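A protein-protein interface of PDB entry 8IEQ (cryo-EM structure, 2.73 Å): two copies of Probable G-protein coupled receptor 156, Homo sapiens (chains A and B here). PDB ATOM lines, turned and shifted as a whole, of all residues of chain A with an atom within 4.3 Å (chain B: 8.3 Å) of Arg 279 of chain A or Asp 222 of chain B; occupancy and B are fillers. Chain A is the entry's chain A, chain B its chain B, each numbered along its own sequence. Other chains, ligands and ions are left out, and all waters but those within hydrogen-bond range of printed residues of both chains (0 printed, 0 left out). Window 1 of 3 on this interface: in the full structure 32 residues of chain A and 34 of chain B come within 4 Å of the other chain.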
ATOM      1  N   ASP A 222      15.023  23.180  -2.982  1.00  0.00           N
ATOM      2  CA  ASP A 222      15.029  23.687  -4.343  1.00  0.00           C
ATOM      3  C   ASP A 222      14.012  24.798  -4.553  1.00  0.00           C
ATOM      4  O   ASP A 222      14.231  25.652  -5.409  1.00  0.00           O
ATOM      5  CB  ASP A 222      14.772  22.548  -5.326  1.00  0.00           C
ATOM      6  CG  ASP A 222      15.945  21.598  -5.427  1.00  0.00           C
ATOM      7  OD1 ASP A 222      17.000  22.009  -5.947  1.00  0.00           O
ATOM      8  OD2 ASP A 222      15.816  20.442  -4.978  1.00  0.00           O
ATOM      9  N   ILE A 225      15.811  27.836  -3.238  1.00  0.00           N
ATOM     10  CA  ILE A 225      16.837  28.130  -4.234  1.00  0.00           C
ATOM     11  C   ILE A 225      16.218  28.828  -5.436  1.00  0.00           C
ATOM     12  O   ILE A 225      16.715  29.859  -5.898  1.00  0.00           O
ATOM     13  CB  ILE A 225      17.565  26.831  -4.639  1.00  0.00           C
ATOM     14  CG1 ILE A 225      18.474  26.355  -3.504  1.00  0.00           C
ATOM     15  CG2 ILE A 225      18.349  27.007  -5.942  1.00  0.00           C
ATOM     16  CD1 ILE A 225      18.930  24.918  -3.641  1.00  0.00           C
ATOM     17  N   PHE A 275      26.509  26.011  -6.964  1.00  0.00           N
ATOM     18  CA  PHE A 275      25.311  25.208  -6.751  1.00  0.00           C
ATOM     19  C   PHE A 275      25.561  23.756  -7.136  1.00  0.00           C
ATOM     20  O   PHE A 275      25.302  22.840  -6.347  1.00  0.00           O
ATOM     21  CB  PHE A 275      24.149  25.794  -7.558  1.00  0.00           C
ATOM     22  CG  PHE A 275      22.954  24.884  -7.663  1.00  0.00           C
ATOM     23  CD1 PHE A 275      22.163  24.622  -6.559  1.00  0.00           C
ATOM     24  CD2 PHE A 275      22.623  24.292  -8.868  1.00  0.00           C
ATOM     25  CE1 PHE A 275      21.068  23.787  -6.657  1.00  0.00           C
ATOM     26  CE2 PHE A 275      21.531  23.457  -8.968  1.00  0.00           C
ATOM     27  CZ  PHE A 275      20.753  23.207  -7.860  1.00  0.00           C
ATOM     28  N   VAL A 276      26.104  23.530  -8.336  1.00  0.00           N
ATOM     29  CA  VAL A 276      26.343  22.159  -8.787  1.00  0.00           C
ATOM     30  C   VAL A 276      27.362  21.468  -7.885  1.00  0.00           C
ATOM     31  O   VAL A 276      27.171  20.319  -7.464  1.00  0.00           O
ATOM     32  CB  VAL A 276      26.796  22.154 -10.258  1.00  0.00           C
ATOM     33  CG1 VAL A 276      27.433  20.821 -10.636  1.00  0.00           C
ATOM     34  CG2 VAL A 276      25.627  22.446 -11.159  1.00  0.00           C
ATOM     35  N   VAL A 277      28.462  22.159  -7.575  1.00  0.00           N
ATOM     36  CA  VAL A 277      29.546  21.540  -6.821  1.00  0.00           C
ATOM     37  C   VAL A 277      29.082  21.180  -5.415  1.00  0.00           C
ATOM     38  O   VAL A 277      29.371  20.087  -4.917  1.00  0.00           O
ATOM     39  CB  VAL A 277      30.771  22.472  -6.805  1.00  0.00           C
ATOM     40  CG1 VAL A 277      31.755  22.078  -5.711  1.00  0.00           C
ATOM     41  CG2 VAL A 277      31.452  22.458  -8.162  1.00  0.00           C
ATOM     42  N   THR A 278      28.364  22.086  -4.749  1.00  0.00           N
ATOM     43  CA  THR A 278      27.836  21.768  -3.430  1.00  0.00           C
ATOM     44  C   THR A 278      26.807  20.650  -3.497  1.00  0.00           C
ATOM     45  O   THR A 278      26.756  19.805  -2.599  1.00  0.00           O
ATOM     46  CB  THR A 278      27.215  23.014  -2.798  1.00  0.00           C
ATOM     47  OG1 THR A 278      28.056  24.147  -3.049  1.00  0.00           O
ATOM     48  CG2 THR A 278      27.056  22.829  -1.301  1.00  0.00           C
ATOM     49  N   ARG A 279      25.980  20.626  -4.547  1.00  0.00           N
ATOM     50  CA  ARG A 279      24.963  19.588  -4.657  1.00  0.00           C
ATOM     51  C   ARG A 279      25.592  18.207  -4.779  1.00  0.00           C
ATOM     52  O   ARG A 279      25.165  17.269  -4.095  1.00  0.00           O
ATOM     53  CB  ARG A 279      24.059  19.887  -5.857  1.00  0.00           C
ATOM     54  CG  ARG A 279      22.989  18.842  -6.173  1.00  0.00           C
ATOM     55  CD  ARG A 279      22.038  18.611  -5.016  1.00  0.00           C
ATOM     56  NE  ARG A 279      21.327  19.827  -4.638  1.00  0.00           N
ATOM     57  CZ  ARG A 279      20.171  20.233  -5.149  1.00  0.00           C
ATOM     58  NH1 ARG A 279      19.556  19.557  -6.105  1.00  0.00           N
ATOM     59  NH2 ARG A 279      19.618  21.350  -4.689  1.00  0.00           N
ATOM     60  N   TYR A 280      26.615  18.062  -5.621  1.00  0.00           N
ATOM     61  CA  TYR A 280      27.131  16.743  -5.976  1.00  0.00           C
ATOM     62  C   TYR A 280      28.463  16.399  -5.325  1.00  0.00           C
ATOM     63  O   TYR A 280      28.640  15.262  -4.874  1.00  0.00           O
ATOM     64  CB  TYR A 280      27.262  16.630  -7.495  1.00  0.00           C
ATOM     65  CG  TYR A 280      25.922  16.498  -8.167  1.00  0.00           C
ATOM     66  CD1 TYR A 280      25.187  15.329  -8.058  1.00  0.00           C
ATOM     67  CD2 TYR A 280      25.377  17.548  -8.882  1.00  0.00           C
ATOM     68  CE1 TYR A 280      23.959  15.205  -8.653  1.00  0.00           C
ATOM     69  CE2 TYR A 280      24.150  17.433  -9.478  1.00  0.00           C
ATOM     70  CZ  TYR A 280      23.442  16.259  -9.363  1.00  0.00           C
ATOM     71  OH  TYR A 280      22.212  16.125  -9.957  1.00  0.00           O
ATOM     72  N   LEU A 281      29.406  17.331  -5.264  1.00  0.00           N
ATOM     73  CA  LEU A 281      30.724  17.049  -4.694  1.00  0.00           C
ATOM     74  C   LEU A 281      30.766  17.377  -3.205  1.00  0.00           C
ATOM     75  O   LEU A 281      31.638  18.096  -2.727  1.00  0.00           O
ATOM     76  CB  LEU A 281      31.795  17.816  -5.462  1.00  0.00           C
ATOM     77  CG  LEU A 281      32.200  17.235  -6.819  1.00  0.00           C
ATOM     78  CD1 LEU A 281      31.113  17.427  -7.862  1.00  0.00           C
ATOM     79  CD2 LEU A 281      33.498  17.861  -7.282  1.00  0.00           C
ATOM     80  N   HIS A 282      29.809  16.840  -2.449  1.00  0.00           N
ATOM     81  CA  HIS A 282      29.780  17.057  -1.007  1.00  0.00           C
ATOM     82  C   HIS A 282      30.802  16.210  -0.262  1.00  0.00           C
ATOM     83  O   HIS A 282      31.088  16.503   0.904  1.00  0.00           O
ATOM     84  CB  HIS A 282      28.382  16.778  -0.442  1.00  0.00           C
ATOM     85  CG  HIS A 282      27.866  15.404  -0.734  1.00  0.00           C
ATOM     86  ND1 HIS A 282      27.126  15.112  -1.860  1.00  0.00           N
ATOM     87  CD2 HIS A 282      27.982  14.242  -0.050  1.00  0.00           C
ATOM     88  CE1 HIS A 282      26.808  13.829  -1.856  1.00  0.00           C
ATOM     89  NE2 HIS A 282      27.317  13.279  -0.769  1.00  0.00           N
ATOM     90  N   ASP B 187      24.648  10.831 -19.831  1.00  0.00           N
ATOM     91  CA  ASP B 187      23.768  10.577 -18.691  1.00  0.00           C
ATOM     92  C   ASP B 187      22.319  10.636 -19.162  1.00  0.00           C
ATOM     93  O   ASP B 187      21.583  11.572 -18.826  1.00  0.00           O
ATOM     94  CB  ASP B 187      24.036  11.590 -17.579  1.00  0.00           C
ATOM     95  CG  ASP B 187      23.421  11.193 -16.256  1.00  0.00           C
ATOM     96  OD1 ASP B 187      22.995  10.029 -16.112  1.00  0.00           O
ATOM     97  OD2 ASP B 187      23.370  12.051 -15.353  1.00  0.00           O
ATOM     98  N   ALA B 217      14.531  10.364 -14.663  1.00  0.00           N
ATOM     99  CA  ALA B 217      15.471  11.471 -14.576  1.00  0.00           C
ATOM    100  C   ALA B 217      16.874  10.935 -14.816  1.00  0.00           C
ATOM    101  O   ALA B 217      17.095   9.725 -14.887  1.00  0.00           O
ATOM    102  CB  ALA B 217      15.383  12.177 -13.221  1.00  0.00           C
ATOM    103  N   SER B 218      17.818  11.860 -14.945  1.00  0.00           N
ATOM    104  CA  SER B 218      19.221  11.510 -15.074  1.00  0.00           C
ATOM    105  C   SER B 218      19.854  11.333 -13.699  1.00  0.00           C
ATOM    106  O   SER B 218      19.351  11.818 -12.683  1.00  0.00           O
ATOM    107  CB  SER B 218      19.973  12.585 -15.853  1.00  0.00           C
ATOM    108  OG  SER B 218      19.511  12.672 -17.183  1.00  0.00           O
ATOM    109  N   ARG B 219      20.983  10.623 -13.677  1.00  0.00           N
ATOM    110  CA  ARG B 219      21.732  10.471 -12.437  1.00  0.00           C
ATOM    111  C   ARG B 219      22.275  11.807 -11.949  1.00  0.00           C
ATOM    112  O   ARG B 219      22.301  12.059 -10.739  1.00  0.00           O
ATOM    113  CB  ARG B 219      22.870   9.474 -12.635  1.00  0.00           C
ATOM    114  CG  ARG B 219      23.500   8.985 -11.340  1.00  0.00           C
ATOM    115  CD  ARG B 219      24.521   7.884 -11.585  1.00  0.00           C
ATOM    116  NE  ARG B 219      25.490   8.239 -12.615  1.00  0.00           N
ATOM    117  CZ  ARG B 219      26.292   7.382 -13.233  1.00  0.00           C
ATOM    118  NH1 ARG B 219      26.284   6.089 -12.942  1.00  0.00           N
ATOM    119  NH2 ARG B 219      27.126   7.830 -14.166  1.00  0.00           N
ATOM    120  N   TYR B 220      22.702  12.669 -12.873  1.00  0.00           N
ATOM    121  CA  TYR B 220      23.270  13.974 -12.551  1.00  0.00           C
ATOM    122  C   TYR B 220      22.419  15.071 -13.177  1.00  0.00           C
ATOM    123  O   TYR B 220      22.940  15.962 -13.851  1.00  0.00           O
ATOM    124  CB  TYR B 220      24.713  14.067 -13.043  1.00  0.00           C
ATOM    125  CG  TYR B 220      25.672  13.215 -12.253  1.00  0.00           C
ATOM    126  CD1 TYR B 220      26.206  13.665 -11.057  1.00  0.00           C
ATOM    127  CD2 TYR B 220      26.052  11.962 -12.709  1.00  0.00           C
ATOM    128  CE1 TYR B 220      27.082  12.887 -10.333  1.00  0.00           C
ATOM    129  CE2 TYR B 220      26.927  11.179 -11.994  1.00  0.00           C
ATOM    130  CZ  TYR B 220      27.440  11.645 -10.807  1.00  0.00           C
ATOM    131  OH  TYR B 220      28.317  10.865 -10.091  1.00  0.00           O
ATOM    132  N   SER B 221      21.102  14.996 -12.971  1.00  0.00           N
ATOM    133  CA  SER B 221      20.175  15.873 -13.680  1.00  0.00           C
ATOM    134  C   SER B 221      20.434  17.344 -13.380  1.00  0.00           C
ATOM    135  O   SER B 221      20.334  18.193 -14.275  1.00  0.00           O
ATOM    136  CB  SER B 221      18.739  15.509 -13.312  1.00  0.00           C
ATOM    137  OG  SER B 221      18.530  15.631 -11.918  1.00  0.00           O
ATOM    138  N   ASP B 222      20.750  17.671 -12.126  1.00  0.00           N
ATOM    139  CA  ASP B 222      20.976  19.066 -11.766  1.00  0.00           C
ATOM    140  C   ASP B 222      22.194  19.650 -12.470  1.00  0.00           C
ATOM    141  O   ASP B 222      22.247  20.860 -12.681  1.00  0.00           O
ATOM    142  CB  ASP B 222      21.115  19.207 -10.251  1.00  0.00           C
ATOM    143  CG  ASP B 222      19.787  19.130  -9.532  1.00  0.00           C
ATOM    144  OD1 ASP B 222      18.804  19.715 -10.025  1.00  0.00           O
ATOM    145  OD2 ASP B 222      19.724  18.477  -8.473  1.00  0.00           O
ATOM    146  N   VAL B 223      23.171  18.827 -12.855  1.00  0.00           N
ATOM    147  CA  VAL B 223      24.314  19.349 -13.603  1.00  0.00           C
ATOM    148  C   VAL B 223      23.860  19.862 -14.963  1.00  0.00           C
ATOM    149  O   VAL B 223      24.210  20.974 -15.383  1.00  0.00           O
ATOM    150  CB  VAL B 223      25.407  18.273 -13.742  1.00  0.00           C
ATOM    151  CG1 VAL B 223      26.618  18.833 -14.476  1.00  0.00           C
ATOM    152  CG2 VAL B 223      25.801  17.750 -12.372  1.00  0.00           C
ATOM    153  N   TRP B 224      23.044  19.069 -15.658  1.00  0.00           N
ATOM    154  CA  TRP B 224      22.557  19.476 -16.972  1.00  0.00           C
ATOM    155  C   TRP B 224      21.599  20.655 -16.854  1.00  0.00           C
ATOM    156  O   TRP B 224      21.596  21.552 -17.702  1.00  0.00           O
ATOM    157  CB  TRP B 224      21.892  18.286 -17.664  1.00  0.00           C
ATOM    158  CG  TRP B 224      22.716  17.042 -17.626  1.00  0.00           C
ATOM    159  CD1 TRP B 224      22.447  15.917 -16.912  1.00  0.00           C
ATOM    160  CD2 TRP B 224      23.934  16.788 -18.336  1.00  0.00           C
ATOM    161  NE1 TRP B 224      23.423  14.980 -17.120  1.00  0.00           N
ATOM    162  CE2 TRP B 224      24.347  15.488 -17.994  1.00  0.00           C
ATOM    163  CE3 TRP B 224      24.715  17.533 -19.224  1.00  0.00           C
ATOM    164  CZ2 TRP B 224      25.506  14.916 -18.507  1.00  0.00           C
ATOM    165  CZ3 TRP B 224      25.864  16.963 -19.732  1.00  0.00           C
ATOM    166  CH2 TRP B 224      26.249  15.668 -19.372  1.00  0.00           C
ATOM    167  N   ILE B 225      20.790  20.670 -15.792  1.00  0.00           N
ATOM    168  CA  ILE B 225      19.908  21.801 -15.514  1.00  0.00           C
ATOM    169  C   ILE B 225      20.714  23.073 -15.308  1.00  0.00           C
ATOM    170  O   ILE B 225      20.470  24.104 -15.949  1.00  0.00           O
ATOM    171  CB  ILE B 225      19.032  21.486 -14.287  1.00  0.00           C
ATOM    172  CG1 ILE B 225      17.972  20.451 -14.677  1.00  0.00           C
ATOM    173  CG2 ILE B 225      18.442  22.743 -13.635  1.00  0.00           C
ATOM    174  CD1 ILE B 225      17.500  19.619 -13.529  1.00  0.00           C
ATOM    175  N   ALA B 226      21.701  23.019 -14.422  1.00  0.00           N
ATOM    176  CA  ALA B 226      22.504  24.203 -14.180  1.00  0.00           C
ATOM    177  C   ALA B 226      23.190  24.654 -15.457  1.00  0.00           C
ATOM    178  O   ALA B 226      23.267  25.851 -15.724  1.00  0.00           O
ATOM    179  CB  ALA B 226      23.525  23.935 -13.082  1.00  0.00           C
ATOM    180  N   LEU B 227      23.637  23.712 -16.287  1.00  0.00           N
ATOM    181  CA  LEU B 227      24.299  24.084 -17.535  1.00  0.00           C
ATOM    182  C   LEU B 227      23.353  24.804 -18.496  1.00  0.00           C
ATOM    183  O   LEU B 227      23.716  25.833 -19.076  1.00  0.00           O
ATOM    184  CB  LEU B 227      24.894  22.840 -18.194  1.00  0.00           C
ATOM    185  CG  LEU B 227      26.350  22.518 -17.844  1.00  0.00           C
ATOM    186  CD1 LEU B 227      26.732  21.177 -18.437  1.00  0.00           C
ATOM    187  CD2 LEU B 227      27.305  23.600 -18.331  1.00  0.00           C
ATOM    188  N   ILE B 228      22.136  24.283 -18.682  1.00  0.00           N
ATOM    189  CA  ILE B 228      21.255  24.829 -19.719  1.00  0.00           C
ATOM    190  C   ILE B 228      20.622  26.141 -19.261  1.00  0.00           C
ATOM    191  O   ILE B 228      20.668  27.152 -19.972  1.00  0.00           O
ATOM    192  CB  ILE B 228      20.195  23.786 -20.118  1.00  0.00           C
ATOM    193  CG1 ILE B 228      20.892  22.634 -20.853  1.00  0.00           C
ATOM    194  CG2 ILE B 228      19.076  24.450 -20.949  1.00  0.00           C
ATOM    195  CD1 ILE B 228      20.011  21.473 -21.233  1.00  0.00           C
ATOM    196  N   TRP B 229      19.977  26.128 -18.092  1.00  0.00           N
ATOM    197  CA  TRP B 229      19.721  27.367 -17.359  1.00  0.00           C
ATOM    198  C   TRP B 229      20.884  28.365 -17.363  1.00  0.00           C
ATOM    199  O   TRP B 229      20.660  29.548 -17.635  1.00  0.00           O
ATOM    200  CB  TRP B 229      19.211  26.986 -15.965  1.00  0.00           C
ATOM    201  CG  TRP B 229      17.752  26.451 -15.939  1.00  0.00           C
ATOM    202  CD1 TRP B 229      16.685  27.262 -15.722  1.00  0.00           C
ATOM    203  CD2 TRP B 229      17.172  25.197 -16.412  1.00  0.00           C
ATOM    204  NE1 TRP B 229      15.516  26.592 -15.835  1.00  0.00           N
ATOM    205  CE2 TRP B 229      15.770  25.327 -16.282  1.00  0.00           C
ATOM    206  CE3 TRP B 229      17.683  23.973 -16.862  1.00  0.00           C
ATOM    207  CZ2 TRP B 229      14.886  24.287 -16.569  1.00  0.00           C
ATOM    208  CZ3 TRP B 229      16.797  22.935 -17.127  1.00  0.00           C
ATOM    209  CH2 TRP B 229      15.421  23.105 -16.992  1.00  0.00           C
ATOM    210  N   PHE B 275      10.240  24.217 -13.079  1.00  0.00           N
ATOM    211  CA  PHE B 275      11.248  23.368 -12.453  1.00  0.00           C
ATOM    212  C   PHE B 275      10.797  22.917 -11.069  1.00  0.00           C
ATOM    213  O   PHE B 275      10.826  21.720 -10.752  1.00  0.00           O
ATOM    214  CB  PHE B 275      12.569  24.135 -12.376  1.00  0.00           C
ATOM    215  CG  PHE B 275      13.625  23.468 -11.537  1.00  0.00           C
ATOM    216  CD1 PHE B 275      14.096  22.208 -11.855  1.00  0.00           C
ATOM    217  CD2 PHE B 275      14.149  24.112 -10.427  1.00  0.00           C
ATOM    218  CE1 PHE B 275      15.066  21.604 -11.084  1.00  0.00           C
ATOM    219  CE2 PHE B 275      15.114  23.508  -9.654  1.00  0.00           C
ATOM    220  CZ  PHE B 275      15.574  22.255  -9.984  1.00  0.00           C
ATOM    221  N   ARG B 279       9.571  19.165  -9.940  1.00  0.00           N
ATOM    222  CA  ARG B 279      10.387  18.447  -8.970  1.00  0.00           C
ATOM    223  C   ARG B 279       9.558  17.960  -7.788  1.00  0.00           C
ATOM    224  O   ARG B 279       9.698  16.807  -7.365  1.00  0.00           O
ATOM    225  CB  ARG B 279      11.529  19.339  -8.491  1.00  0.00           C
ATOM    226  CG  ARG B 279      12.514  18.650  -7.568  1.00  0.00           C
ATOM    227  CD  ARG B 279      13.673  19.563  -7.259  1.00  0.00           C
ATOM    228  NE  ARG B 279      14.656  19.545  -8.337  1.00  0.00           N
ATOM    229  CZ  ARG B 279      15.755  18.800  -8.369  1.00  0.00           C
ATOM    230  NH1 ARG B 279      16.093  18.006  -7.365  1.00  0.00           N
ATOM    231  NH2 ARG B 279      16.538  18.853  -9.442  1.00  0.00           N
ATOM    232  N   TYR B 280       8.688  18.812  -7.247  1.00  0.00           N
ATOM    233  CA  TYR B 280       8.017  18.521  -5.983  1.00  0.00           C
ATOM    234  C   TYR B 280       6.586  18.026  -6.139  1.00  0.00           C
ATOM    235  O   TYR B 280       6.188  17.100  -5.429  1.00  0.00           O
ATOM    236  CB  TYR B 280       8.037  19.763  -5.084  1.00  0.00           C
ATOM    237  CG  TYR B 280       9.408  20.059  -4.515  1.00  0.00           C
ATOM    238  CD1 TYR B 280      10.084  19.116  -3.753  1.00  0.00           C
ATOM    239  CD2 TYR B 280      10.034  21.271  -4.753  1.00  0.00           C
ATOM    240  CE1 TYR B 280      11.330  19.370  -3.246  1.00  0.00           C
ATOM    241  CE2 TYR B 280      11.285  21.535  -4.245  1.00  0.00           C
ATOM    242  CZ  TYR B 280      11.927  20.578  -3.492  1.00  0.00           C
ATOM    243  OH  TYR B 280      13.172  20.824  -2.976  1.00  0.00           O
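Asp 222 of chain A touches Arg 279 of chain B, and with the chains exchanged Arg 279 of chain A touches Asp 222 of chain B. Asp 222 of chain A touches Tyr 280 of chain B, and with the chains exchanged Tyr 280 of chain A touches Asp 222 of chain B. Arg 279 of chain A touches its own counterpart, Arg 279 of chain B. Of the 10 pairs that touch across the chains among the printed residues, 5 have their exchanged pair printed and touching as well.
OD2 of Asp 187 of chain B lies within hydrogen-bond range of N of Tyr 220 of chain B (2.6 Å). The indole nitrogen (NE1) of Trp 224 of chain B sits close to the backbone carbonyl oxygen (O) of Tyr 220 of chain B (3.4 Å). The guanidinium group of Arg 279 of chain B is in salt-bridge range of the side-chain carboxylate of Asp 222 of chain B (2.5 Å). ND1 of His 282 of chain A lies within hydrogen-bond range of O of Tyr 280 of chain A, at 3.4 Å. OD1 of Asp 222 of chain A lies within salt-bridge range of NH2 of Arg 279 of chain A, 3.0 Å away.
Of the 17 printed residues of chain B, 7 touch a printed residue of chain A. Hydrophobic or aromatic side chains of chain B that line the printed part of chain A: Tyr 220, Val 223, Ala 226 and Tyr 280. Of the 10 printed residues of chain A, 4 touch a printed residue of chain B. Among the printed residues, Asp or Glu carboxylates within 4 Å of a Lys or Arg side-chain nitrogen of the other chain: Asp 222 of chain A with Arg 279 of chain B (3.4 Å) and Arg 279 of chain A with Asp 222 of chain B (2.6 Å).
Of the printed residues of chain B, Val 276 of chain A touches Val 223 (3.9 Å) and Ala 226 (3.2 Å). Printed residues of chain B within 4 Å of Arg 279 of chain A: Asp 222 and Arg 279. Of the printed residues of chain B, Tyr 280 of chain A touches Tyr 220 (3.4 Å), Ser 221 (3.4 Å), Asp 222 (3.0 Å) and Val 223 (3.3 Å). His 282 of chain A touches none of the printed residues of chain B. Asp 222 of chain B touches just these residues of chain A: Arg 279 (2.6 Å) and Tyr 280 (3.0 Å). Of the printed residues of chain A, Val 223 of chain B touches Val 276 (3.9 Å) and Tyr 280 (3.3 Å). Of the printed residues of chain A, Arg 279 of chain B touches Asp 222 (3.3 Å) and Arg 279 (3.998 Å). Printed residues of chain A within 4 Å of Tyr 280 of chain B: Asp 222. The nearest printed residue of chain B that does not touch Arg 279 of chain A is Phe 275 of chain B (6.2 Å). The nearest printed residue of chain A that does not touch Tyr 280 of chain B is Arg 279 of chain A (6.7 Å).
The side-chain hydroxyl of Tyr 280 of chain A lies within hydrogen-bond range of the backbone NH of Ser 221 of chain B (3.4 Å). NH1 of Arg 279 of chain B is in salt-bridge range of OD2 of Asp 222 of chain A, 3.4 Å away. The guanidinium group of Arg 279 of chain A lies within salt-bridge range of the side-chain carboxylate of Asp 222 of chain B. N of Asp 222 of chain A lies within hydrogen-bond range of OH of Tyr 280 of chain B, at 3.0 Å. The side-chain hydroxyl (OH) of Tyr 280 of chain A sits at hydrogen-bond distance from the backbone NH (N) of Asp 222 of chain B.
Among the printed residues, pairs that only touch across the chains: Val 276 of chain A with Val 223 of chain B (3.9 Å), Val 276 of chain A with Ala 226 of chain B (3.2 Å), Arg 279 of chain A with Arg 279 of chain B (3.998 Å), Tyr 280 of chain A with Tyr 220 of chain B (3.4 Å) and Tyr 280 of chain A with Val 223 of chain B (3.3 Å).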
